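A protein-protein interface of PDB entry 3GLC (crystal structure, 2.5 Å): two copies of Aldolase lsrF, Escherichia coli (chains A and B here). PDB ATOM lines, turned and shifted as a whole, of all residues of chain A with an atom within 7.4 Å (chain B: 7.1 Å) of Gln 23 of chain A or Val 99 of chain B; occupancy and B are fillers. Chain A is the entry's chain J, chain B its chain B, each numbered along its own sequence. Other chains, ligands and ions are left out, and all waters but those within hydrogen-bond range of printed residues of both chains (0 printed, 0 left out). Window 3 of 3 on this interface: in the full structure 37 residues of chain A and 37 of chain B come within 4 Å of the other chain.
NH1 of Arg 74 of chain B sits at hydrogen-bond distance from O of Arg 18 of chain A. The backbone carbonyl oxygen of Gln 21 of chain A lies within hydrogen-bond range of the guanidinium group of Arg 74 of chain B (2.9 Å). The indole nitrogen (NE1) of Trp 38 of chain A sits at hydrogen-bond distance from the backbone carbonyl oxygen (O) of Leu 96 of chain B (3.4 Å). The backbone carbonyl oxygen (O) of Val 100 of chain B sits at hydrogen-bond distance from the indole nitrogen (NE1) of Trp 38 of chain A, 2.8 Å away. The guanidinium group (NH2) of Arg 74 of chain B sits close to the backbone NH (N) of Gln 23 of chain A (3.4 Å).
The guanidinium group (NH2) of Arg 74 of chain B is in salt-bridge range of the side-chain carboxylate (OD2) of Asp 76 of chain B (2.9 Å). The backbone NH (N) of Val 100 of chain B lies within hydrogen-bond range of the backbone carbonyl oxygen (O) of Ile 95 of chain B (3.4 Å). The side-chain hydroxyl (OG1) of Thr 104 of chain B is in hydrogen-bond range of the backbone carbonyl oxygen (O) of Pro 101 of chain B, at 2.5 Å. NH2 of Arg 18 of chain A sits at hydrogen-bond distance from OE1 of Gln 21 of chain A, at 2.8 Å.
Arg 18 of chain A touches Ile 77 of chain B (NH1 to CG2, 3.8 Å). Arg 74 of chain B touches Pro 22 of chain A. Asp 76 of chain B touches Gln 23 of chain A. Val 99 of chain B touches Gln 23 of chain A (CG1 to NE2, 3.3 Å). CD1 of Ile 26 of chain A touches CG of Pro 101 of chain B (3.7 Å). NE1 of Trp 38 of chain A touches N of Pro 102 of chain B, 3.5 Å away.
Of the printed residues of chain B, Arg 18 of chain A touches Arg 74 (3.0 Å) and Ile 77 (3.8 Å). Printed residues of chain B within 4 Å of Gln 21 of chain A: Arg 74. Printed residues of chain A within 4 Å of Arg 74 of chain B: Arg 18, Gln 21, Pro 22 and Gln 23. Printed residues of chain A within 4 Å of Ile 77 of chain B: Arg 18 (3.8 Å). Val 99 of chain B touches just one residue of chain A: Gln 23. Thr 104 of chain B touches none of the printed residues of chain A. The nearest residue of chain B that does not touch Gln 23 of chain A is Ser 98 of chain B (4.2 Å). The nearest printed residue of chain A that does not touch Pro 102 of chain B is Ile 26 of chain A (5.7 Å).
Of the 18 printed residues of chain B, 8 touch a printed residue of chain A. Hydrophobic or aromatic side chains of chain B within 4 Å of the printed part of chain A: Ile 77, Leu 96, Val 99, Pro 101 and Pro 102. Hydrophobic or aromatic side chains of chain A within 4 Å of the printed part of chain B: Ile 26 and Trp 38.
No position is printed for both chains. Of the 11 pairs that touch across the chains among the printed residues, none has its exchanged pair printed and touching as well.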
ATOM      1  N   ARG A  18       5.787  25.522   6.720  1.00  0.00           N
ATOM      2  CA  ARG A  18       5.254  26.808   6.255  1.00  0.00           C
ATOM      3  C   ARG A  18       3.742  26.830   6.368  1.00  0.00           C
ATOM      4  O   ARG A  18       3.025  27.144   5.424  1.00  0.00           O
ATOM      5  CB  ARG A  18       5.692  27.079   4.815  1.00  0.00           C
ATOM      6  CG  ARG A  18       7.194  26.823   4.571  1.00  0.00           C
ATOM      7  CD  ARG A  18       7.815  28.013   3.869  1.00  0.00           C
ATOM      8  NE  ARG A  18       7.020  29.198   4.196  1.00  0.00           N
ATOM      9  CZ  ARG A  18       6.939  30.290   3.451  1.00  0.00           C
ATOM     10  NH1 ARG A  18       7.621  30.393   2.319  1.00  0.00           N
ATOM     11  NH2 ARG A  18       6.166  31.284   3.852  1.00  0.00           N
ATOM     12  N   GLN A  21       1.340  29.577   5.151  1.00  0.00           N
ATOM     13  CA  GLN A  21       1.101  29.810   3.733  1.00  0.00           C
ATOM     14  C   GLN A  21       0.434  28.612   3.054  1.00  0.00           C
ATOM     15  O   GLN A  21       1.091  27.622   2.749  1.00  0.00           O
ATOM     16  CB  GLN A  21       2.399  30.162   3.039  1.00  0.00           C
ATOM     17  CG  GLN A  21       2.208  30.659   1.614  1.00  0.00           C
ATOM     18  CD  GLN A  21       3.522  31.094   0.960  1.00  0.00           C
ATOM     19  OE1 GLN A  21       4.519  31.359   1.645  1.00  0.00           O
ATOM     20  NE2 GLN A  21       3.526  31.167  -0.371  1.00  0.00           N
ATOM     21  N   PRO A  22      -0.876  28.712   2.784  1.00  0.00           N
ATOM     22  CA  PRO A  22      -1.605  27.527   2.325  1.00  0.00           C
ATOM     23  C   PRO A  22      -1.304  27.223   0.857  1.00  0.00           C
ATOM     24  O   PRO A  22      -1.042  28.141   0.073  1.00  0.00           O
ATOM     25  CB  PRO A  22      -3.090  27.907   2.530  1.00  0.00           C
ATOM     26  CG  PRO A  22      -3.080  29.380   3.054  1.00  0.00           C
ATOM     27  CD  PRO A  22      -1.716  29.922   2.735  1.00  0.00           C
ATOM     28  N   GLN A  23      -1.308  25.938   0.512  1.00  0.00           N
ATOM     29  CA  GLN A  23      -1.048  25.496  -0.851  1.00  0.00           C
ATOM     30  C   GLN A  23      -2.076  26.091  -1.797  1.00  0.00           C
ATOM     31  O   GLN A  23      -3.219  26.256  -1.444  1.00  0.00           O
ATOM     32  CB  GLN A  23      -1.061  23.962  -0.905  1.00  0.00           C
ATOM     33  CG  GLN A  23      -0.915  23.351  -2.277  1.00  0.00           C
ATOM     34  CD  GLN A  23      -0.831  21.865  -2.189  1.00  0.00           C
ATOM     35  OE1 GLN A  23      -0.299  21.348  -1.219  1.00  0.00           O
ATOM     36  NE2 GLN A  23      -1.366  21.157  -3.192  1.00  0.00           N
ATOM     37  N   LYS A  24      -1.656  26.421  -3.006  1.00  0.00           N
ATOM     38  CA  LYS A  24      -2.584  26.998  -3.970  1.00  0.00           C
ATOM     39  C   LYS A  24      -2.415  26.402  -5.371  1.00  0.00           C
ATOM     40  O   LYS A  24      -1.307  26.326  -5.873  1.00  0.00           O
ATOM     41  CB  LYS A  24      -2.395  28.516  -3.993  1.00  0.00           C
ATOM     42  CG  LYS A  24      -3.568  29.282  -4.528  1.00  0.00           C
ATOM     43  CD  LYS A  24      -3.331  30.796  -4.523  1.00  0.00           C
ATOM     44  CE  LYS A  24      -4.321  31.500  -5.485  1.00  0.00           C
ATOM     45  NZ  LYS A  24      -4.411  32.972  -5.268  1.00  0.00           N
ATOM     46  N   ASN A  25      -3.503  25.958  -5.999  1.00  0.00           N
ATOM     47  CA  ASN A  25      -3.382  25.416  -7.356  1.00  0.00           C
ATOM     48  C   ASN A  25      -2.990  26.490  -8.360  1.00  0.00           C
ATOM     49  O   ASN A  25      -3.503  27.605  -8.319  1.00  0.00           O
ATOM     50  CB  ASN A  25      -4.682  24.768  -7.827  1.00  0.00           C
ATOM     51  CG  ASN A  25      -5.081  23.579  -7.004  1.00  0.00           C
ATOM     52  OD1 ASN A  25      -4.280  23.032  -6.243  1.00  0.00           O
ATOM     53  ND2 ASN A  25      -6.347  23.169  -7.142  1.00  0.00           N
ATOM     54  N   ILE A  26      -2.099  26.134  -9.268  1.00  0.00           N
ATOM     55  CA  ILE A  26      -1.741  27.019 -10.358  1.00  0.00           C
ATOM     56  C   ILE A  26      -2.606  26.782 -11.616  1.00  0.00           C
ATOM     57  O   ILE A  26      -2.555  25.698 -12.218  1.00  0.00           O
ATOM     58  CB  ILE A  26      -0.225  26.924 -10.668  1.00  0.00           C
ATOM     59  CG1 ILE A  26       0.554  27.582  -9.543  1.00  0.00           C
ATOM     60  CG2 ILE A  26       0.109  27.649 -11.954  1.00  0.00           C
ATOM     61  CD1 ILE A  26       1.989  27.185  -9.485  1.00  0.00           C
ATOM     62  N   TRP A  38      -3.370  15.681 -16.287  1.00  0.00           N
ATOM     63  CA  TRP A  38      -2.014  16.178 -16.337  1.00  0.00           C
ATOM     64  C   TRP A  38      -1.333  15.870 -17.664  1.00  0.00           C
ATOM     65  O   TRP A  38      -0.867  16.798 -18.379  1.00  0.00           O
ATOM     66  CB  TRP A  38      -1.219  15.674 -15.139  1.00  0.00           C
ATOM     67  CG  TRP A  38       0.013  16.432 -14.895  1.00  0.00           C
ATOM     68  CD1 TRP A  38       0.206  17.418 -13.961  1.00  0.00           C
ATOM     69  CD2 TRP A  38       1.262  16.277 -15.571  1.00  0.00           C
ATOM     70  NE1 TRP A  38       1.497  17.938 -14.048  1.00  0.00           N
ATOM     71  CE2 TRP A  38       2.171  17.243 -15.018  1.00  0.00           C
ATOM     72  CE3 TRP A  38       1.714  15.433 -16.593  1.00  0.00           C
ATOM     73  CZ2 TRP A  38       3.509  17.358 -15.448  1.00  0.00           C
ATOM     74  CZ3 TRP A  38       3.034  15.562 -17.029  1.00  0.00           C
ATOM     75  CH2 TRP A  38       3.911  16.535 -16.462  1.00  0.00           C
ATOM     76  N   PHE B  60      13.028  14.575  -6.578  1.00  0.00           N
ATOM     77  CA  PHE B  60      12.302  14.839  -5.345  1.00  0.00           C
ATOM     78  C   PHE B  60      11.195  13.781  -5.084  1.00  0.00           C
ATOM     79  O   PHE B  60      10.076  14.095  -4.661  1.00  0.00           O
ATOM     80  CB  PHE B  60      11.765  16.283  -5.348  1.00  0.00           C
ATOM     81  CG  PHE B  60      10.995  16.663  -6.591  1.00  0.00           C
ATOM     82  CD1 PHE B  60       9.618  16.725  -6.575  1.00  0.00           C
ATOM     83  CD2 PHE B  60      11.648  16.989  -7.760  1.00  0.00           C
ATOM     84  CE1 PHE B  60       8.880  17.100  -7.727  1.00  0.00           C
ATOM     85  CE2 PHE B  60      10.949  17.365  -8.926  1.00  0.00           C
ATOM     86  CZ  PHE B  60       9.563  17.419  -8.916  1.00  0.00           C
ATOM     87  N   ARG B  74       7.346  21.113   1.513  1.00  0.00           N
ATOM     88  CA  ARG B  74       6.437  21.889   0.650  1.00  0.00           C
ATOM     89  C   ARG B  74       6.976  22.016  -0.767  1.00  0.00           C
ATOM     90  O   ARG B  74       7.626  23.014  -1.112  1.00  0.00           O
ATOM     91  CB  ARG B  74       6.186  23.289   1.236  1.00  0.00           C
ATOM     92  CG  ARG B  74       5.500  23.310   2.607  1.00  0.00           C
ATOM     93  CD  ARG B  74       4.074  22.823   2.486  1.00  0.00           C
ATOM     94  NE  ARG B  74       3.307  23.656   1.556  1.00  0.00           N
ATOM     95  CZ  ARG B  74       2.626  24.733   1.920  1.00  0.00           C
ATOM     96  NH1 ARG B  74       2.616  25.126   3.183  1.00  0.00           N
ATOM     97  NH2 ARG B  74       1.966  25.416   1.019  1.00  0.00           N
ATOM     98  N   ILE B  75       6.710  21.005  -1.588  1.00  0.00           N
ATOM     99  CA  ILE B  75       7.231  20.958  -2.940  1.00  0.00           C
ATOM    100  C   ILE B  75       6.687  22.146  -3.666  1.00  0.00           C
ATOM    101  O   ILE B  75       7.360  22.736  -4.501  1.00  0.00           O
ATOM    102  CB  ILE B  75       6.770  19.697  -3.681  1.00  0.00           C
ATOM    103  CG1 ILE B  75       7.098  18.432  -2.869  1.00  0.00           C
ATOM    104  CG2 ILE B  75       7.355  19.625  -5.091  1.00  0.00           C
ATOM    105  CD1 ILE B  75       8.479  17.937  -2.991  1.00  0.00           C
ATOM    106  N   ASP B  76       5.465  22.516  -3.339  1.00  0.00           N
ATOM    107  CA  ASP B  76       4.785  23.610  -4.058  1.00  0.00           C
ATOM    108  C   ASP B  76       5.433  24.996  -3.883  1.00  0.00           C
ATOM    109  O   ASP B  76       5.257  25.886  -4.730  1.00  0.00           O
ATOM    110  CB  ASP B  76       3.310  23.695  -3.651  1.00  0.00           C
ATOM    111  CG  ASP B  76       3.119  23.919  -2.140  1.00  0.00           C
ATOM    112  OD1 ASP B  76       3.723  23.173  -1.313  1.00  0.00           O
ATOM    113  OD2 ASP B  76       2.326  24.835  -1.786  1.00  0.00           O
ATOM    114  N   ILE B  77       6.151  25.186  -2.779  1.00  0.00           N
ATOM    115  CA  ILE B  77       6.712  26.486  -2.484  1.00  0.00           C
ATOM    116  C   ILE B  77       8.221  26.459  -2.676  1.00  0.00           C
ATOM    117  O   ILE B  77       8.813  27.334  -3.306  1.00  0.00           O
ATOM    118  CB  ILE B  77       6.417  26.867  -1.046  1.00  0.00           C
ATOM    119  CG1 ILE B  77       4.908  27.040  -0.857  1.00  0.00           C
ATOM    120  CG2 ILE B  77       7.215  28.127  -0.660  1.00  0.00           C
ATOM    121  CD1 ILE B  77       4.503  27.216   0.573  1.00  0.00           C
ATOM    122  N   ALA B  80       9.210  24.185  -6.442  1.00  0.00           N
ATOM    123  CA  ALA B  80       8.604  24.691  -7.666  1.00  0.00           C
ATOM    124  C   ALA B  80       9.482  25.713  -8.414  1.00  0.00           C
ATOM    125  O   ALA B  80       9.629  25.619  -9.646  1.00  0.00           O
ATOM    126  CB  ALA B  80       7.194  25.252  -7.383  1.00  0.00           C
ATOM    127  N   PHE B  83      12.136  24.162 -10.889  1.00  0.00           N
ATOM    128  CA  PHE B  83      11.845  23.316 -12.044  1.00  0.00           C
ATOM    129  C   PHE B  83      12.502  23.836 -13.295  1.00  0.00           C
ATOM    130  O   PHE B  83      13.205  23.091 -13.961  1.00  0.00           O
ATOM    131  CB  PHE B  83      10.349  23.168 -12.299  1.00  0.00           C
ATOM    132  CG  PHE B  83       9.602  22.532 -11.185  1.00  0.00           C
ATOM    133  CD1 PHE B  83      10.192  21.550 -10.406  1.00  0.00           C
ATOM    134  CD2 PHE B  83       8.282  22.898 -10.928  1.00  0.00           C
ATOM    135  CE1 PHE B  83       9.507  20.957  -9.370  1.00  0.00           C
ATOM    136  CE2 PHE B  83       7.571  22.279  -9.907  1.00  0.00           C
ATOM    137  CZ  PHE B  83       8.193  21.298  -9.120  1.00  0.00           C
ATOM    138  N   ARG B  93       3.811  10.018  -9.241  1.00  0.00           N
ATOM    139  CA  ARG B  93       2.617  10.472  -9.929  1.00  0.00           C
ATOM    140  C   ARG B  93       1.719  11.251  -8.980  1.00  0.00           C
ATOM    141  O   ARG B  93       0.967  12.136  -9.398  1.00  0.00           O
ATOM    142  CB  ARG B  93       1.864   9.304 -10.557  1.00  0.00           C
ATOM    143  CG  ARG B  93       1.209   8.355  -9.572  1.00  0.00           C
ATOM    144  CD  ARG B  93       0.256   7.372 -10.291  1.00  0.00           C
ATOM    145  NE  ARG B  93      -0.055   6.197  -9.474  1.00  0.00           N
ATOM    146  CZ  ARG B  93      -0.662   5.093  -9.938  1.00  0.00           C
ATOM    147  NH1 ARG B  93      -1.046   5.010 -11.217  1.00  0.00           N
ATOM    148  NH2 ARG B  93      -0.897   4.063  -9.115  1.00  0.00           N
ATOM    149  N   GLY B  94       1.818  10.953  -7.693  1.00  0.00           N
ATOM    150  CA  GLY B  94       1.040  11.707  -6.713  1.00  0.00           C
ATOM    151  C   GLY B  94       1.478  13.156  -6.620  1.00  0.00           C
ATOM    152  O   GLY B  94       0.639  14.073  -6.628  1.00  0.00           O
ATOM    153  N   ILE B  95       2.807  13.370  -6.539  1.00  0.00           N
ATOM    154  CA  ILE B  95       3.342  14.733  -6.455  1.00  0.00           C
ATOM    155  C   ILE B  95       3.157  15.427  -7.794  1.00  0.00           C
ATOM    156  O   ILE B  95       2.764  16.609  -7.868  1.00  0.00           O
ATOM    157  CB  ILE B  95       4.802  14.717  -6.015  1.00  0.00           C
ATOM    158  CG1 ILE B  95       4.911  14.375  -4.526  1.00  0.00           C
ATOM    159  CG2 ILE B  95       5.500  16.046  -6.293  1.00  0.00           C
ATOM    160  CD1 ILE B  95       4.006  15.223  -3.631  1.00  0.00           C
ATOM    161  N   LEU B  96       3.364  14.670  -8.857  1.00  0.00           N
ATOM    162  CA  LEU B  96       3.235  15.211 -10.193  1.00  0.00           C
ATOM    163  C   LEU B  96       1.876  15.823 -10.404  1.00  0.00           C
ATOM    164  O   LEU B  96       1.806  17.008 -10.753  1.00  0.00           O
ATOM    165  CB  LEU B  96       3.528  14.151 -11.264  1.00  0.00           C
ATOM    166  CG  LEU B  96       3.680  14.710 -12.677  1.00  0.00           C
ATOM    167  CD1 LEU B  96       4.904  15.583 -12.782  1.00  0.00           C
ATOM    168  CD2 LEU B  96       3.760  13.602 -13.692  1.00  0.00           C
ATOM    169  N   ARG B  97       0.815  15.052 -10.163  1.00  0.00           N
ATOM    170  CA  ARG B  97      -0.524  15.501 -10.468  1.00  0.00           C
ATOM    171  C   ARG B  97      -0.955  16.577  -9.525  1.00  0.00           C
ATOM    172  O   ARG B  97      -1.730  17.427  -9.905  1.00  0.00           O
ATOM    173  CB  ARG B  97      -1.557  14.346 -10.436  1.00  0.00           C
ATOM    174  CG  ARG B  97      -1.711  13.560 -11.725  1.00  0.00           C
ATOM    175  CD  ARG B  97      -2.942  12.655 -11.701  1.00  0.00           C
ATOM    176  NE  ARG B  97      -2.603  11.301 -12.130  1.00  0.00           N
ATOM    177  CZ  ARG B  97      -2.793  10.830 -13.357  1.00  0.00           C
ATOM    178  NH1 ARG B  97      -3.362  11.586 -14.258  1.00  0.00           N
ATOM    179  NH2 ARG B  97      -2.457   9.597 -13.675  1.00  0.00           N
ATOM    180  N   SER B  98      -0.496  16.532  -8.290  1.00  0.00           N
ATOM    181  CA  SER B  98      -1.040  17.442  -7.293  1.00  0.00           C
ATOM    182  C   SER B  98      -0.355  18.824  -7.283  1.00  0.00           C
ATOM    183  O   SER B  98      -1.055  19.851  -7.141  1.00  0.00           O
ATOM    184  CB  SER B  98      -1.059  16.826  -5.875  1.00  0.00           C
ATOM    185  OG  SER B  98       0.243  16.600  -5.358  1.00  0.00           O
ATOM    186  N   VAL B  99       0.980  18.865  -7.439  1.00  0.00           N
ATOM    187  CA  VAL B  99       1.700  20.137  -7.263  1.00  0.00           C
ATOM    188  C   VAL B  99       2.743  20.504  -8.314  1.00  0.00           C
ATOM    189  O   VAL B  99       3.348  21.542  -8.200  1.00  0.00           O
ATOM    190  CB  VAL B  99       2.394  20.249  -5.882  1.00  0.00           C
ATOM    191  CG1 VAL B  99       1.371  20.315  -4.761  1.00  0.00           C
ATOM    192  CG2 VAL B  99       3.377  19.105  -5.674  1.00  0.00           C
ATOM    193  N   VAL B 100       2.981  19.672  -9.310  1.00  0.00           N
ATOM    194  CA  VAL B 100       3.867  20.061 -10.368  1.00  0.00           C
ATOM    195  C   VAL B 100       2.985  20.576 -11.482  1.00  0.00           C
ATOM    196  O   VAL B 100       2.299  19.754 -12.110  1.00  0.00           O
ATOM    197  CB  VAL B 100       4.679  18.869 -10.890  1.00  0.00           C
ATOM    198  CG1 VAL B 100       5.541  19.269 -12.073  1.00  0.00           C
ATOM    199  CG2 VAL B 100       5.543  18.278  -9.772  1.00  0.00           C
ATOM    200  N   PRO B 101       2.981  21.914 -11.732  1.00  0.00           N
ATOM    201  CA  PRO B 101       2.148  22.487 -12.776  1.00  0.00           C
ATOM    202  C   PRO B 101       2.484  21.881 -14.129  1.00  0.00           C
ATOM    203  O   PRO B 101       3.652  21.839 -14.523  1.00  0.00           O
ATOM    204  CB  PRO B 101       2.538  23.985 -12.774  1.00  0.00           C
ATOM    205  CG  PRO B 101       3.015  24.229 -11.392  1.00  0.00           C
ATOM    206  CD  PRO B 101       3.735  22.957 -11.019  1.00  0.00           C
ATOM    207  N   PRO B 102       1.466  21.388 -14.847  1.00  0.00           N
ATOM    208  CA  PRO B 102       1.800  20.834 -16.174  1.00  0.00           C
ATOM    209  C   PRO B 102       2.449  21.858 -17.086  1.00  0.00           C
ATOM    210  O   PRO B 102       3.115  21.476 -18.038  1.00  0.00           O
ATOM    211  CB  PRO B 102       0.438  20.412 -16.738  1.00  0.00           C
ATOM    212  CG  PRO B 102      -0.580  21.053 -15.813  1.00  0.00           C
ATOM    213  CD  PRO B 102       0.052  21.176 -14.483  1.00  0.00           C
ATOM    214  N   THR B 104       4.859  23.643 -16.544  1.00  0.00           N
ATOM    215  CA  THR B 104       6.297  23.552 -16.337  1.00  0.00           C
ATOM    216  C   THR B 104       7.040  23.127 -17.581  1.00  0.00           C
ATOM    217  O   THR B 104       8.178  23.523 -17.775  1.00  0.00           O
ATOM    218  CB  THR B 104       6.608  22.549 -15.246  1.00  0.00           C
ATOM    219  OG1 THR B 104       5.894  22.933 -14.079  1.00  0.00           O
ATOM    220  CG2 THR B 104       8.111  22.504 -14.929  1.00  0.00           C
